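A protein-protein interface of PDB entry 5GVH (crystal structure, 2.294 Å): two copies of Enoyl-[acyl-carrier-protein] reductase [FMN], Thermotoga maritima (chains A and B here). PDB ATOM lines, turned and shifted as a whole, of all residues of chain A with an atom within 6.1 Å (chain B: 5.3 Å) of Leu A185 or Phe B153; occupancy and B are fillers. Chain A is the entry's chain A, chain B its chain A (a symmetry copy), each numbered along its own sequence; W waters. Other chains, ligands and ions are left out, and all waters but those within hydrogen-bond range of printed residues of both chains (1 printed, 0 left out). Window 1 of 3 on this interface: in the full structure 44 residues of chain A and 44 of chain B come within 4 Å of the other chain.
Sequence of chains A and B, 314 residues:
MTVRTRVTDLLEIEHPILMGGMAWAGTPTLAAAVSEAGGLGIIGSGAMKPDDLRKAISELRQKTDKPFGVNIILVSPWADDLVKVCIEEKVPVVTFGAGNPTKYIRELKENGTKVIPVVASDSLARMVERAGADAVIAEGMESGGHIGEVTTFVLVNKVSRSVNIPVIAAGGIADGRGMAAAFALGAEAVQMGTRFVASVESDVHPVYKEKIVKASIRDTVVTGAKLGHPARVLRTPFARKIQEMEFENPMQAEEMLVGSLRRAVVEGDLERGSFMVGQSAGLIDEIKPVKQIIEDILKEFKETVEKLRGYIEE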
ATOM      1  N   GLU A 142     -13.966   3.100 -13.279  1.00  0.00           N
ATOM      2  CA  GLU A 142     -12.633   2.514 -13.179  1.00  0.00           C
ATOM      3  C   GLU A 142     -12.400   1.392 -14.184  1.00  0.00           C
ATOM      4  O   GLU A 142     -11.291   0.852 -14.236  1.00  0.00           O
ATOM      5  CB  GLU A 142     -12.363   1.992 -11.761  1.00  0.00           C
ATOM      6  CG  GLU A 142     -13.398   1.029 -11.206  1.00  0.00           C
ATOM      7  CD  GLU A 142     -14.558   1.760 -10.552  1.00  0.00           C
ATOM      8  OE1 GLU A 142     -15.302   2.452 -11.283  1.00  0.00           O
ATOM      9  OE2 GLU A 142     -14.696   1.673  -9.306  1.00  0.00           O
ATOM     10  N   THR A 152     -17.850   2.224  -9.598  1.00  0.00           N
ATOM     11  CA  THR A 152     -18.464   0.930  -9.293  1.00  0.00           C
ATOM     12  C   THR A 152     -19.082   0.909  -7.899  1.00  0.00           C
ATOM     13  O   THR A 152     -20.197   0.405  -7.718  1.00  0.00           O
ATOM     14  CB  THR A 152     -17.420  -0.184  -9.426  1.00  0.00           C
ATOM     15  OG1 THR A 152     -17.064  -0.337 -10.806  1.00  0.00           O
ATOM     16  CG2 THR A 152     -17.941  -1.502  -8.879  1.00  0.00           C
ATOM     17  N   PHE A 153     -18.374   1.456  -6.901  1.00  0.00           N
ATOM     18  CA  PHE A 153     -18.852   1.386  -5.526  1.00  0.00           C
ATOM     19  C   PHE A 153     -20.216   2.042  -5.377  1.00  0.00           C
ATOM     20  O   PHE A 153     -21.071   1.538  -4.641  1.00  0.00           O
ATOM     21  CB  PHE A 153     -17.838   2.044  -4.588  1.00  0.00           C
ATOM     22  CG  PHE A 153     -17.898   1.539  -3.173  1.00  0.00           C
ATOM     23  CD1 PHE A 153     -17.046   0.529  -2.746  1.00  0.00           C
ATOM     24  CD2 PHE A 153     -18.801   2.074  -2.267  1.00  0.00           C
ATOM     25  CE1 PHE A 153     -17.096   0.055  -1.431  1.00  0.00           C
ATOM     26  CE2 PHE A 153     -18.850   1.617  -0.941  1.00  0.00           C
ATOM     27  CZ  PHE A 153     -17.999   0.604  -0.528  1.00  0.00           C
ATOM     28  N   VAL A 154     -20.439   3.157  -6.067  1.00  0.00           N
ATOM     29  CA  VAL A 154     -21.724   3.840  -6.018  1.00  0.00           C
ATOM     30  C   VAL A 154     -22.710   3.272  -7.038  1.00  0.00           C
ATOM     31  O   VAL A 154     -23.868   3.018  -6.700  1.00  0.00           O
ATOM     32  CB  VAL A 154     -21.518   5.356  -6.213  1.00  0.00           C
ATOM     33  CG1 VAL A 154     -22.855   6.048  -6.389  1.00  0.00           C
ATOM     34  CG2 VAL A 154     -20.777   5.956  -5.022  1.00  0.00           C
ATOM     35  N   VAL A 156     -23.156   0.305  -8.644  1.00  0.00           N
ATOM     36  CA  VAL A 156     -23.748  -1.004  -8.371  1.00  0.00           C
ATOM     37  C   VAL A 156     -24.771  -0.905  -7.249  1.00  0.00           C
ATOM     38  O   VAL A 156     -25.846  -1.515  -7.314  1.00  0.00           O
ATOM     39  CB  VAL A 156     -22.655  -2.038  -8.044  1.00  0.00           C
ATOM     40  CG1 VAL A 156     -23.280  -3.391  -7.703  1.00  0.00           C
ATOM     41  CG2 VAL A 156     -21.695  -2.176  -9.216  1.00  0.00           C
ATOM     42  N   ASN A 157     -24.458  -0.131  -6.207  1.00  0.00           N
ATOM     43  CA  ASN A 157     -25.394   0.051  -5.103  1.00  0.00           C
ATOM     44  C   ASN A 157     -26.708   0.644  -5.598  1.00  0.00           C
ATOM     45  O   ASN A 157     -27.782   0.056  -5.411  1.00  0.00           O
ATOM     46  CB  ASN A 157     -24.757   0.951  -4.035  1.00  0.00           C
ATOM     47  CG  ASN A 157     -25.547   0.978  -2.747  1.00  0.00           C
ATOM     48  OD1 ASN A 157     -26.666   0.467  -2.673  1.00  0.00           O
ATOM     49  ND2 ASN A 157     -24.967   1.585  -1.714  1.00  0.00           N
ATOM     50  N   LYS A 158     -26.631   1.805  -6.257  1.00  0.00           N
ATOM     51  CA  LYS A 158     -27.821   2.531  -6.685  1.00  0.00           C
ATOM     52  C   LYS A 158     -28.628   1.755  -7.736  1.00  0.00           C
ATOM     53  O   LYS A 158     -29.863   1.702  -7.657  1.00  0.00           O
ATOM     54  CB  LYS A 158     -27.402   3.901  -7.214  1.00  0.00           C
ATOM     55  CG  LYS A 158     -28.537   4.758  -7.725  1.00  0.00           C
ATOM     56  CD  LYS A 158     -29.570   4.948  -6.639  1.00  0.00           C
ATOM     57  CE  LYS A 158     -30.699   5.824  -7.103  1.00  0.00           C
ATOM     58  NZ  LYS A 158     -31.681   5.905  -6.003  1.00  0.00           N
ATOM     59  N   SER A 160     -28.821  -1.563  -8.305  1.00  0.00           N
ATOM     60  CA  SER A 160     -29.486  -2.705  -7.670  1.00  0.00           C
ATOM     61  C   SER A 160     -30.817  -2.324  -7.021  1.00  0.00           C
ATOM     62  O   SER A 160     -31.797  -3.074  -7.118  1.00  0.00           O
ATOM     63  CB  SER A 160     -28.574  -3.324  -6.614  1.00  0.00           C
ATOM     64  OG  SER A 160     -27.548  -4.094  -7.193  1.00  0.00           O
ATOM     65  N   ALA A 169     -22.049  -6.521 -11.686  1.00  0.00           N
ATOM     66  CA  ALA A 169     -21.083  -5.469 -11.422  1.00  0.00           C
ATOM     67  C   ALA A 169     -19.896  -5.630 -12.351  1.00  0.00           C
ATOM     68  O   ALA A 169     -19.377  -6.737 -12.505  1.00  0.00           O
ATOM     69  CB  ALA A 169     -20.627  -5.520  -9.964  1.00  0.00           C
ATOM     70  N   GLY A 171     -16.112  -3.430 -13.679  1.00  0.00           N
ATOM     71  CA  GLY A 171     -15.207  -2.319 -13.454  1.00  0.00           C
ATOM     72  C   GLY A 171     -14.509  -2.367 -12.108  1.00  0.00           C
ATOM     73  O   GLY A 171     -15.109  -2.099 -11.058  1.00  0.00           O
ATOM     74  N   GLY A 172     -13.227  -2.720 -12.133  1.00  0.00           N
ATOM     75  CA  GLY A 172     -12.439  -2.818 -10.924  1.00  0.00           C
ATOM     76  C   GLY A 172     -12.460  -4.165 -10.231  1.00  0.00           C
ATOM     77  O   GLY A 172     -11.848  -4.288  -9.159  1.00  0.00           O
ATOM     78  N   ILE A 173     -13.138  -5.182 -10.791  1.00  0.00           N
ATOM     79  CA  ILE A 173     -13.200  -6.497 -10.157  1.00  0.00           C
ATOM     80  C   ILE A 173     -12.077  -7.371 -10.706  1.00  0.00           C
ATOM     81  O   ILE A 173     -11.997  -7.614 -11.920  1.00  0.00           O
ATOM     82  CB  ILE A 173     -14.566  -7.176 -10.363  1.00  0.00           C
ATOM     83  CG1 ILE A 173     -15.695  -6.425  -9.659  1.00  0.00           C
ATOM     84  CG2 ILE A 173     -14.532  -8.557  -9.752  1.00  0.00           C
ATOM     85  CD1 ILE A 173     -16.454  -5.453 -10.523  1.00  0.00           C
ATOM     86  N   ALA A 174     -11.222  -7.870  -9.804  1.00  0.00           N
ATOM     87  CA  ALA A 174     -10.108  -8.702 -10.240  1.00  0.00           C
ATOM     88  C   ALA A 174      -9.812  -9.875  -9.319  1.00  0.00           C
ATOM     89  O   ALA A 174      -8.861 -10.614  -9.595  1.00  0.00           O
ATOM     90  CB  ALA A 174      -8.845  -7.844 -10.410  1.00  0.00           C
ATOM     91  N   ARG A 177     -12.241 -10.707  -3.385  1.00  0.00           N
ATOM     92  CA  ARG A 177     -12.726  -9.568  -2.597  1.00  0.00           C
ATOM     93  C   ARG A 177     -13.648  -8.681  -3.420  1.00  0.00           C
ATOM     94  O   ARG A 177     -14.697  -8.239  -2.931  1.00  0.00           O
ATOM     95  CB  ARG A 177     -11.561  -8.734  -2.059  1.00  0.00           C
ATOM     96  CG  ARG A 177     -10.570  -9.486  -1.204  1.00  0.00           C
ATOM     97  CD  ARG A 177      -9.375  -8.604  -0.896  1.00  0.00           C
ATOM     98  NE  ARG A 177      -8.656  -9.044   0.299  1.00  0.00           N
ATOM     99  CZ  ARG A 177      -7.858  -8.266   1.026  1.00  0.00           C
ATOM    100  NH1 ARG A 177      -7.679  -6.994   0.697  1.00  0.00           N
ATOM    101  NH2 ARG A 177      -7.247  -8.759   2.091  1.00  0.00           N
ATOM    102  N   GLY A 178     -13.262  -8.391  -4.665  1.00  0.00           N
ATOM    103  CA  GLY A 178     -14.150  -7.668  -5.560  1.00  0.00           C
ATOM    104  C   GLY A 178     -15.527  -8.300  -5.670  1.00  0.00           C
ATOM    105  O   GLY A 178     -16.543  -7.613  -5.540  1.00  0.00           O
ATOM    106  N   MET A 179     -15.584  -9.621  -5.888  1.00  0.00           N
ATOM    107  CA  MET A 179     -16.877 -10.290  -6.031  1.00  0.00           C
ATOM    108  C   MET A 179     -17.696 -10.145  -4.756  1.00  0.00           C
ATOM    109  O   MET A 179     -18.868  -9.746  -4.799  1.00  0.00           O
ATOM    110  CB  MET A 179     -16.683 -11.773  -6.398  1.00  0.00           C
ATOM    111  CG  MET A 179     -17.863 -12.437  -7.167  1.00  0.00           C
ATOM    112  SD  MET A 179     -17.979 -14.265  -7.081  1.00  0.00           S
ATOM    113  CE  MET A 179     -16.298 -14.626  -7.333  1.00  0.00           C
ATOM    114  N   ALA A 180     -17.081 -10.434  -3.604  1.00  0.00           N
ATOM    115  CA  ALA A 180     -17.772 -10.266  -2.329  1.00  0.00           C
ATOM    116  C   ALA A 180     -18.308  -8.848  -2.172  1.00  0.00           C
ATOM    117  O   ALA A 180     -19.479  -8.654  -1.821  1.00  0.00           O
ATOM    118  CB  ALA A 180     -16.835 -10.621  -1.174  1.00  0.00           C
ATOM    119  N   ALA A 181     -17.475  -7.842  -2.450  1.00  0.00           N
ATOM    120  CA  ALA A 181     -17.915  -6.457  -2.249  1.00  0.00           C
ATOM    121  C   ALA A 181     -19.008  -6.078  -3.238  1.00  0.00           C
ATOM    122  O   ALA A 181     -19.956  -5.365  -2.879  1.00  0.00           O
ATOM    123  CB  ALA A 181     -16.738  -5.491  -2.369  1.00  0.00           C
ATOM    124  N   ALA A 182     -18.884  -6.542  -4.491  1.00  0.00           N
ATOM    125  CA  ALA A 182     -19.917  -6.322  -5.503  1.00  0.00           C
ATOM    126  C   ALA A 182     -21.233  -6.966  -5.101  1.00  0.00           C
ATOM    127  O   ALA A 182     -22.301  -6.356  -5.260  1.00  0.00           O
ATOM    128  CB  ALA A 182     -19.461  -6.883  -6.854  1.00  0.00           C
ATOM    129  N   PHE A 183     -21.175  -8.208  -4.602  1.00  0.00           N
ATOM    130  CA  PHE A 183     -22.363  -8.862  -4.060  1.00  0.00           C
ATOM    131  C   PHE A 183     -22.922  -8.085  -2.874  1.00  0.00           C
ATOM    132  O   PHE A 183     -24.145  -7.907  -2.763  1.00  0.00           O
ATOM    133  CB  PHE A 183     -22.037 -10.305  -3.653  1.00  0.00           C
ATOM    134  CG  PHE A 183     -22.074 -11.297  -4.795  1.00  0.00           C
ATOM    135  CD1 PHE A 183     -22.845 -12.446  -4.706  1.00  0.00           C
ATOM    136  CD2 PHE A 183     -21.346 -11.078  -5.959  1.00  0.00           C
ATOM    137  CE1 PHE A 183     -22.883 -13.357  -5.758  1.00  0.00           C
ATOM    138  CE2 PHE A 183     -21.378 -11.991  -7.010  1.00  0.00           C
ATOM    139  CZ  PHE A 183     -22.142 -13.124  -6.906  1.00  0.00           C
ATOM    140  N   ALA A 184     -22.045  -7.605  -1.975  1.00  0.00           N
ATOM    141  CA  ALA A 184     -22.516  -6.784  -0.861  1.00  0.00           C
ATOM    142  C   ALA A 184     -23.231  -5.537  -1.363  1.00  0.00           C
ATOM    143  O   ALA A 184     -24.225  -5.102  -0.767  1.00  0.00           O
ATOM    144  CB  ALA A 184     -21.355  -6.397   0.058  1.00  0.00           C
ATOM    145  N   LEU A 185     -22.740  -4.949  -2.460  1.00  0.00           N
ATOM    146  CA  LEU A 185     -23.346  -3.745  -3.017  1.00  0.00           C
ATOM    147  C   LEU A 185     -24.678  -4.018  -3.702  1.00  0.00           C
ATOM    148  O   LEU A 185     -25.376  -3.060  -4.061  1.00  0.00           O
ATOM    149  CB  LEU A 185     -22.383  -3.084  -4.004  1.00  0.00           C
ATOM    150  CG  LEU A 185     -21.118  -2.454  -3.414  1.00  0.00           C
ATOM    151  CD1 LEU A 185     -20.170  -1.989  -4.516  1.00  0.00           C
ATOM    152  CD2 LEU A 185     -21.469  -1.295  -2.464  1.00  0.00           C
ATOM    153  N   GLY A 186     -25.039  -5.283  -3.898  1.00  0.00           N
ATOM    154  CA  GLY A 186     -26.313  -5.655  -4.480  1.00  0.00           C
ATOM    155  C   GLY A 186     -26.225  -6.448  -5.765  1.00  0.00           C
ATOM    156  O   GLY A 186     -27.275  -6.856  -6.283  1.00  0.00           O
ATOM    157  N   ALA A 187     -25.034  -6.675  -6.321  1.00  0.00           N
ATOM    158  CA  ALA A 187     -24.910  -7.429  -7.561  1.00  0.00           C
ATOM    159  C   ALA A 187     -25.118  -8.913  -7.300  1.00  0.00           C
ATOM    160  O   ALA A 187     -25.065  -9.386  -6.162  1.00  0.00           O
ATOM    161  CB  ALA A 187     -23.542  -7.210  -8.207  1.00  0.00           C
ATOM    162  N   LEU A 283      -4.236  -4.474  -9.495  1.00  0.00           N
ATOM    163  CA  LEU A 283      -4.547  -5.632  -8.672  1.00  0.00           C
ATOM    164  C   LEU A 283      -4.063  -6.935  -9.293  1.00  0.00           C
ATOM    165  O   LEU A 283      -4.211  -7.991  -8.674  1.00  0.00           O
ATOM    166  CB  LEU A 283      -6.056  -5.712  -8.414  1.00  0.00           C
ATOM    167  CG  LEU A 283      -6.781  -4.402  -8.091  1.00  0.00           C
ATOM    168  CD1 LEU A 283      -8.279  -4.652  -8.040  1.00  0.00           C
ATOM    169  CD2 LEU A 283      -6.291  -3.756  -6.771  1.00  0.00           C
ATOM    170  N   GLU B 142     -14.599   9.078  -5.872  1.00  0.00           N
ATOM    171  CA  GLU B 142     -16.015   9.425  -5.785  1.00  0.00           C
ATOM    172  C   GLU B 142     -16.352  10.244  -4.545  1.00  0.00           C
ATOM    173  O   GLU B 142     -17.508  10.645  -4.385  1.00  0.00           O
ATOM    174  CB  GLU B 142     -16.895   8.167  -5.819  1.00  0.00           C
ATOM    175  CG  GLU B 142     -16.556   7.099  -4.794  1.00  0.00           C
ATOM    176  CD  GLU B 142     -15.466   6.165  -5.290  1.00  0.00           C
ATOM    177  OE1 GLU B 142     -14.321   6.640  -5.467  1.00  0.00           O
ATOM    178  OE2 GLU B 142     -15.767   4.970  -5.539  1.00  0.00           O
ATOM    179  N   THR B 151     -10.479   4.859  -7.699  1.00  0.00           N
ATOM    180  CA  THR B 151     -11.804   4.679  -7.119  1.00  0.00           C
ATOM    181  C   THR B 151     -11.717   3.882  -5.821  1.00  0.00           C
ATOM    182  O   THR B 151     -10.775   3.113  -5.593  1.00  0.00           O
ATOM    183  CB  THR B 151     -12.752   3.947  -8.083  1.00  0.00           C
ATOM    184  OG1 THR B 151     -12.305   2.598  -8.274  1.00  0.00           O
ATOM    185  CG2 THR B 151     -12.842   4.668  -9.440  1.00  0.00           C
ATOM    186  N   THR B 152     -12.733   4.067  -4.974  1.00  0.00           N
ATOM    187  CA  THR B 152     -12.813   3.339  -3.706  1.00  0.00           C
ATOM    188  C   THR B 152     -12.719   1.831  -3.910  1.00  0.00           C
ATOM    189  O   THR B 152     -12.012   1.142  -3.164  1.00  0.00           O
ATOM    190  CB  THR B 152     -14.117   3.696  -2.983  1.00  0.00           C
ATOM    191  OG1 THR B 152     -14.058   5.059  -2.545  1.00  0.00           O
ATOM    192  CG2 THR B 152     -14.361   2.781  -1.795  1.00  0.00           C
ATOM    193  N   PHE B 153     -13.421   1.300  -4.920  1.00  0.00           N
ATOM    194  CA  PHE B 153     -13.463  -0.144  -5.118  1.00  0.00           C
ATOM    195  C   PHE B 153     -12.070  -0.715  -5.333  1.00  0.00           C
ATOM    196  O   PHE B 153     -11.760  -1.802  -4.832  1.00  0.00           O
ATOM    197  CB  PHE B 153     -14.367  -0.481  -6.306  1.00  0.00           C
ATOM    198  CG  PHE B 153     -14.954  -1.864  -6.252  1.00  0.00           C
ATOM    199  CD1 PHE B 153     -16.224  -2.073  -5.730  1.00  0.00           C
ATOM    200  CD2 PHE B 153     -14.241  -2.957  -6.725  1.00  0.00           C
ATOM    201  CE1 PHE B 153     -16.777  -3.358  -5.678  1.00  0.00           C
ATOM    202  CE2 PHE B 153     -14.791  -4.247  -6.692  1.00  0.00           C
ATOM    203  CZ  PHE B 153     -16.058  -4.444  -6.162  1.00  0.00           C
ATOM    204  N   VAL B 154     -11.220  -0.001  -6.065  1.00  0.00           N
ATOM    205  CA  VAL B 154      -9.853  -0.447  -6.299  1.00  0.00           C
ATOM    206  C   VAL B 154      -8.912  -0.010  -5.178  1.00  0.00           C
ATOM    207  O   VAL B 154      -8.118  -0.817  -4.690  1.00  0.00           O
ATOM    208  CB  VAL B 154      -9.368   0.055  -7.674  1.00  0.00           C
ATOM    209  CG1 VAL B 154      -7.883  -0.206  -7.833  1.00  0.00           C
ATOM    210  CG2 VAL B 154     -10.137  -0.630  -8.800  1.00  0.00           C
ATOM    211  N   LEU B 155      -8.986   1.253  -4.732  1.00  0.00           N
ATOM    212  CA  LEU B 155      -7.999   1.766  -3.776  1.00  0.00           C
ATOM    213  C   LEU B 155      -8.021   0.983  -2.467  1.00  0.00           C
ATOM    214  O   LEU B 155      -6.969   0.549  -1.983  1.00  0.00           O
ATOM    215  CB  LEU B 155      -8.233   3.249  -3.505  1.00  0.00           C
ATOM    216  CG  LEU B 155      -7.285   3.975  -2.554  1.00  0.00           C
ATOM    217  CD1 LEU B 155      -5.906   4.184  -3.169  1.00  0.00           C
ATOM    218  CD2 LEU B 155      -7.905   5.290  -2.145  1.00  0.00           C
ATOM    219  N   VAL B 156      -9.211   0.786  -1.882  1.00  0.00           N
ATOM    220  CA  VAL B 156      -9.305   0.092  -0.598  1.00  0.00           C
ATOM    221  C   VAL B 156      -8.729  -1.313  -0.704  1.00  0.00           C
ATOM    222  O   VAL B 156      -8.024  -1.780   0.199  1.00  0.00           O
ATOM    223  CB  VAL B 156     -10.761   0.065  -0.100  1.00  0.00           C
ATOM    224  CG1 VAL B 156     -10.866  -0.710   1.215  1.00  0.00           C
ATOM    225  CG2 VAL B 156     -11.282   1.483   0.077  1.00  0.00           C
ATOM    226  N   ASN B 157      -9.015  -2.005  -1.810  1.00  0.00           N
ATOM    227  CA  ASN B 157      -8.475  -3.344  -2.013  1.00  0.00           C
ATOM    228  C   ASN B 157      -6.951  -3.325  -1.995  1.00  0.00           C
ATOM    229  O   ASN B 157      -6.315  -4.016  -1.187  1.00  0.00           O
ATOM    230  CB  ASN B 157      -8.998  -3.911  -3.340  1.00  0.00           C
ATOM    231  CG  ASN B 157      -8.704  -5.384  -3.504  1.00  0.00           C
ATOM    232  OD1 ASN B 157      -7.964  -5.978  -2.718  1.00  0.00           O
ATOM    233  ND2 ASN B 157      -9.282  -5.988  -4.539  1.00  0.00           N
ATOM    234  N   ARG B 177     -24.648  -1.395   3.120  1.00  0.00           N
ATOM    235  CA  ARG B 177     -24.019  -2.116   2.007  1.00  0.00           C
ATOM    236  C   ARG B 177     -22.614  -1.596   1.737  1.00  0.00           C
ATOM    237  O   ARG B 177     -21.685  -2.385   1.516  1.00  0.00           O
ATOM    238  CB  ARG B 177     -24.859  -2.004   0.733  1.00  0.00           C
ATOM    239  CG  ARG B 177     -26.279  -2.503   0.851  1.00  0.00           C
ATOM    240  CD  ARG B 177     -27.055  -2.163  -0.407  1.00  0.00           C
ATOM    241  NE  ARG B 177     -28.222  -3.027  -0.588  1.00  0.00           N
ATOM    242  CZ  ARG B 177     -28.826  -3.241  -1.753  1.00  0.00           C
ATOM    243  NH1 ARG B 177     -28.373  -2.668  -2.860  1.00  0.00           N
ATOM    244  NH2 ARG B 177     -29.880  -4.039  -1.815  1.00  0.00           N
ATOM    245  N   GLY B 178     -22.448  -0.272   1.726  1.00  0.00           N
ATOM    246  CA  GLY B 178     -21.115   0.299   1.613  1.00  0.00           C
ATOM    247  C   GLY B 178     -20.144  -0.251   2.644  1.00  0.00           C
ATOM    248  O   GLY B 178     -19.034  -0.662   2.298  1.00  0.00           O
ATOM    249  N   ALA B 181     -19.276  -3.861   1.875  1.00  0.00           N
ATOM    250  CA  ALA B 181     -18.407  -3.994   0.701  1.00  0.00           C
ATOM    251  C   ALA B 181     -17.006  -3.474   0.991  1.00  0.00           C
ATOM    252  O   ALA B 181     -16.015  -4.061   0.533  1.00  0.00           O
ATOM    253  CB  ALA B 181     -19.002  -3.261  -0.501  1.00  0.00           C
ATOM    254  N   LEU B 185     -13.576  -5.481   0.895  1.00  0.00           N
ATOM    255  CA  LEU B 185     -12.400  -5.025   0.161  1.00  0.00           C
ATOM    256  C   LEU B 185     -11.147  -4.980   1.023  1.00  0.00           C
ATOM    257  O   LEU B 185     -10.051  -4.780   0.481  1.00  0.00           O
ATOM    258  CB  LEU B 185     -12.663  -3.644  -0.440  1.00  0.00           C
ATOM    259  CG  LEU B 185     -13.688  -3.572  -1.577  1.00  0.00           C
ATOM    260  CD1 LEU B 185     -13.980  -2.124  -1.962  1.00  0.00           C
ATOM    261  CD2 LEU B 185     -13.217  -4.383  -2.797  1.00  0.00           C
HETATM  262  O   HOH W   1     -11.231  -4.107  -6.373  1.00  0.00           O
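The guanidinium group (NH1) of Arg B177 lies within hydrogen-bond range of the backbone carbonyl oxygen (O) of Leu A185, 3.3 Å away. The backbone carbonyl oxygen (O) of Leu B185 sits at hydrogen-bond distance from the guanidinium group (NH1) of Arg A177, at 3.3 Å. The side-chain hydroxyl of Thr B151 is in hydrogen-bond range of the side-chain carboxylate of Glu A142, at 2.8 Å.
The side-chain carboxylate (OE1) of Glu B142 sits at hydrogen-bond distance from the backbone NH (N) of Thr B152 (3.1 Å). N of Ala A187 sits at hydrogen-bond distance from O of Ala A182 (2.9 Å). The side-chain carboxylate (OE1) of Glu A142 is in hydrogen-bond range of the backbone NH (N) of Thr A152 (3.1 Å). The backbone carbonyl oxygen of Gly A186 lies within hydrogen-bond range of the side-chain hydroxyl of Ser A160 (2.9 Å). O of Val A156 is in hydrogen-bond range of OG of Ser A160, 3.1 Å away. OG1 of Thr A152 sits at hydrogen-bond distance from O of Gly A171, 2.6 Å away.
Among the printed residues, merely in contact across the chains: Glu A142 with Phe B153, Thr A152 with Phe B153, Phe A153 with Glu B142, Phe A153 with Thr B152, Phe A153 with Gly B178, Phe A153 with Ala B181, Phe A153 with Leu B185, Asn A157 with Arg B177, Ser A160 with Arg B177, Gly A172 with Phe B153, Gly A172 with Val B154, Ile A173 with Phe B153, Arg A177 with Asn B157, Gly A178 with Phe B153, Ala A181 with Phe B153, Ala A181 with Ala B181, Ala A181 with Leu B185, Ala A182 with Phe B153, Ala A184 with Arg B177, Ala A184 with Ala B181, Leu A185 with Phe B153, Leu A185 with Ala B181, Gly A186 with Arg B177 and Leu A283 with Asn B157.
Of chain B, only Phe B153, Arg B177 and Ala B181 come within 4 Å of Leu A185. Of the printed residues of chain B, Ile A173 touches Phe B153 (3.8 Å). Printed residues of chain A within 4 Å of Val B154: Gly A172 (3.8 Å). Of the printed residues of chain A, Asn B157 touches Arg A177 and Leu A283. Of the printed residues of chain B, Arg A177 touches Asn B157 (3.5 Å) and Leu B185 (3.3 Å). Of the printed residues of chain A, Thr B151 touches Glu A142. The nearest residue of chain A that does not touch Phe B153 is Phe A153 (4.04 Å).
Printed residues of chain B that touch a printed residue of chain A: Glu B142, Thr B151, Thr B152, Phe B153, Val B154, Asn B157, Arg B177, Gly B178, Ala B181 and Leu B185. Of the 25 printed residues of chain A, 15 touch a printed residue of chain B. Among the printed residues, 27 pairs touch across the chains. Among the printed residues, no Asp or Glu carboxylate lies within 4 Å of a Lys or Arg side-chain nitrogen of the other chain.
Glu A142 touches Phe B153, and with the chains exchanged Phe A153 touches Glu B142. Phe A153 touches Ala B181, and with the chains exchanged Ala A181 touches Phe B153. Ala B181 touches its own counterpart, Ala A181. Ala A181 touches Leu B185, and with the chains exchanged Leu A185 touches Ala B181. Of the 27 pairs that touch across the chains among the printed residues, 17 have their exchanged pair printed and touching as well.
Water W1 lies within hydrogen-bond range of O of Phe B153 (2.8 Å), O of Gly A172 (2.9 Å) and ND2 of Asn B157 (3.3 Å).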
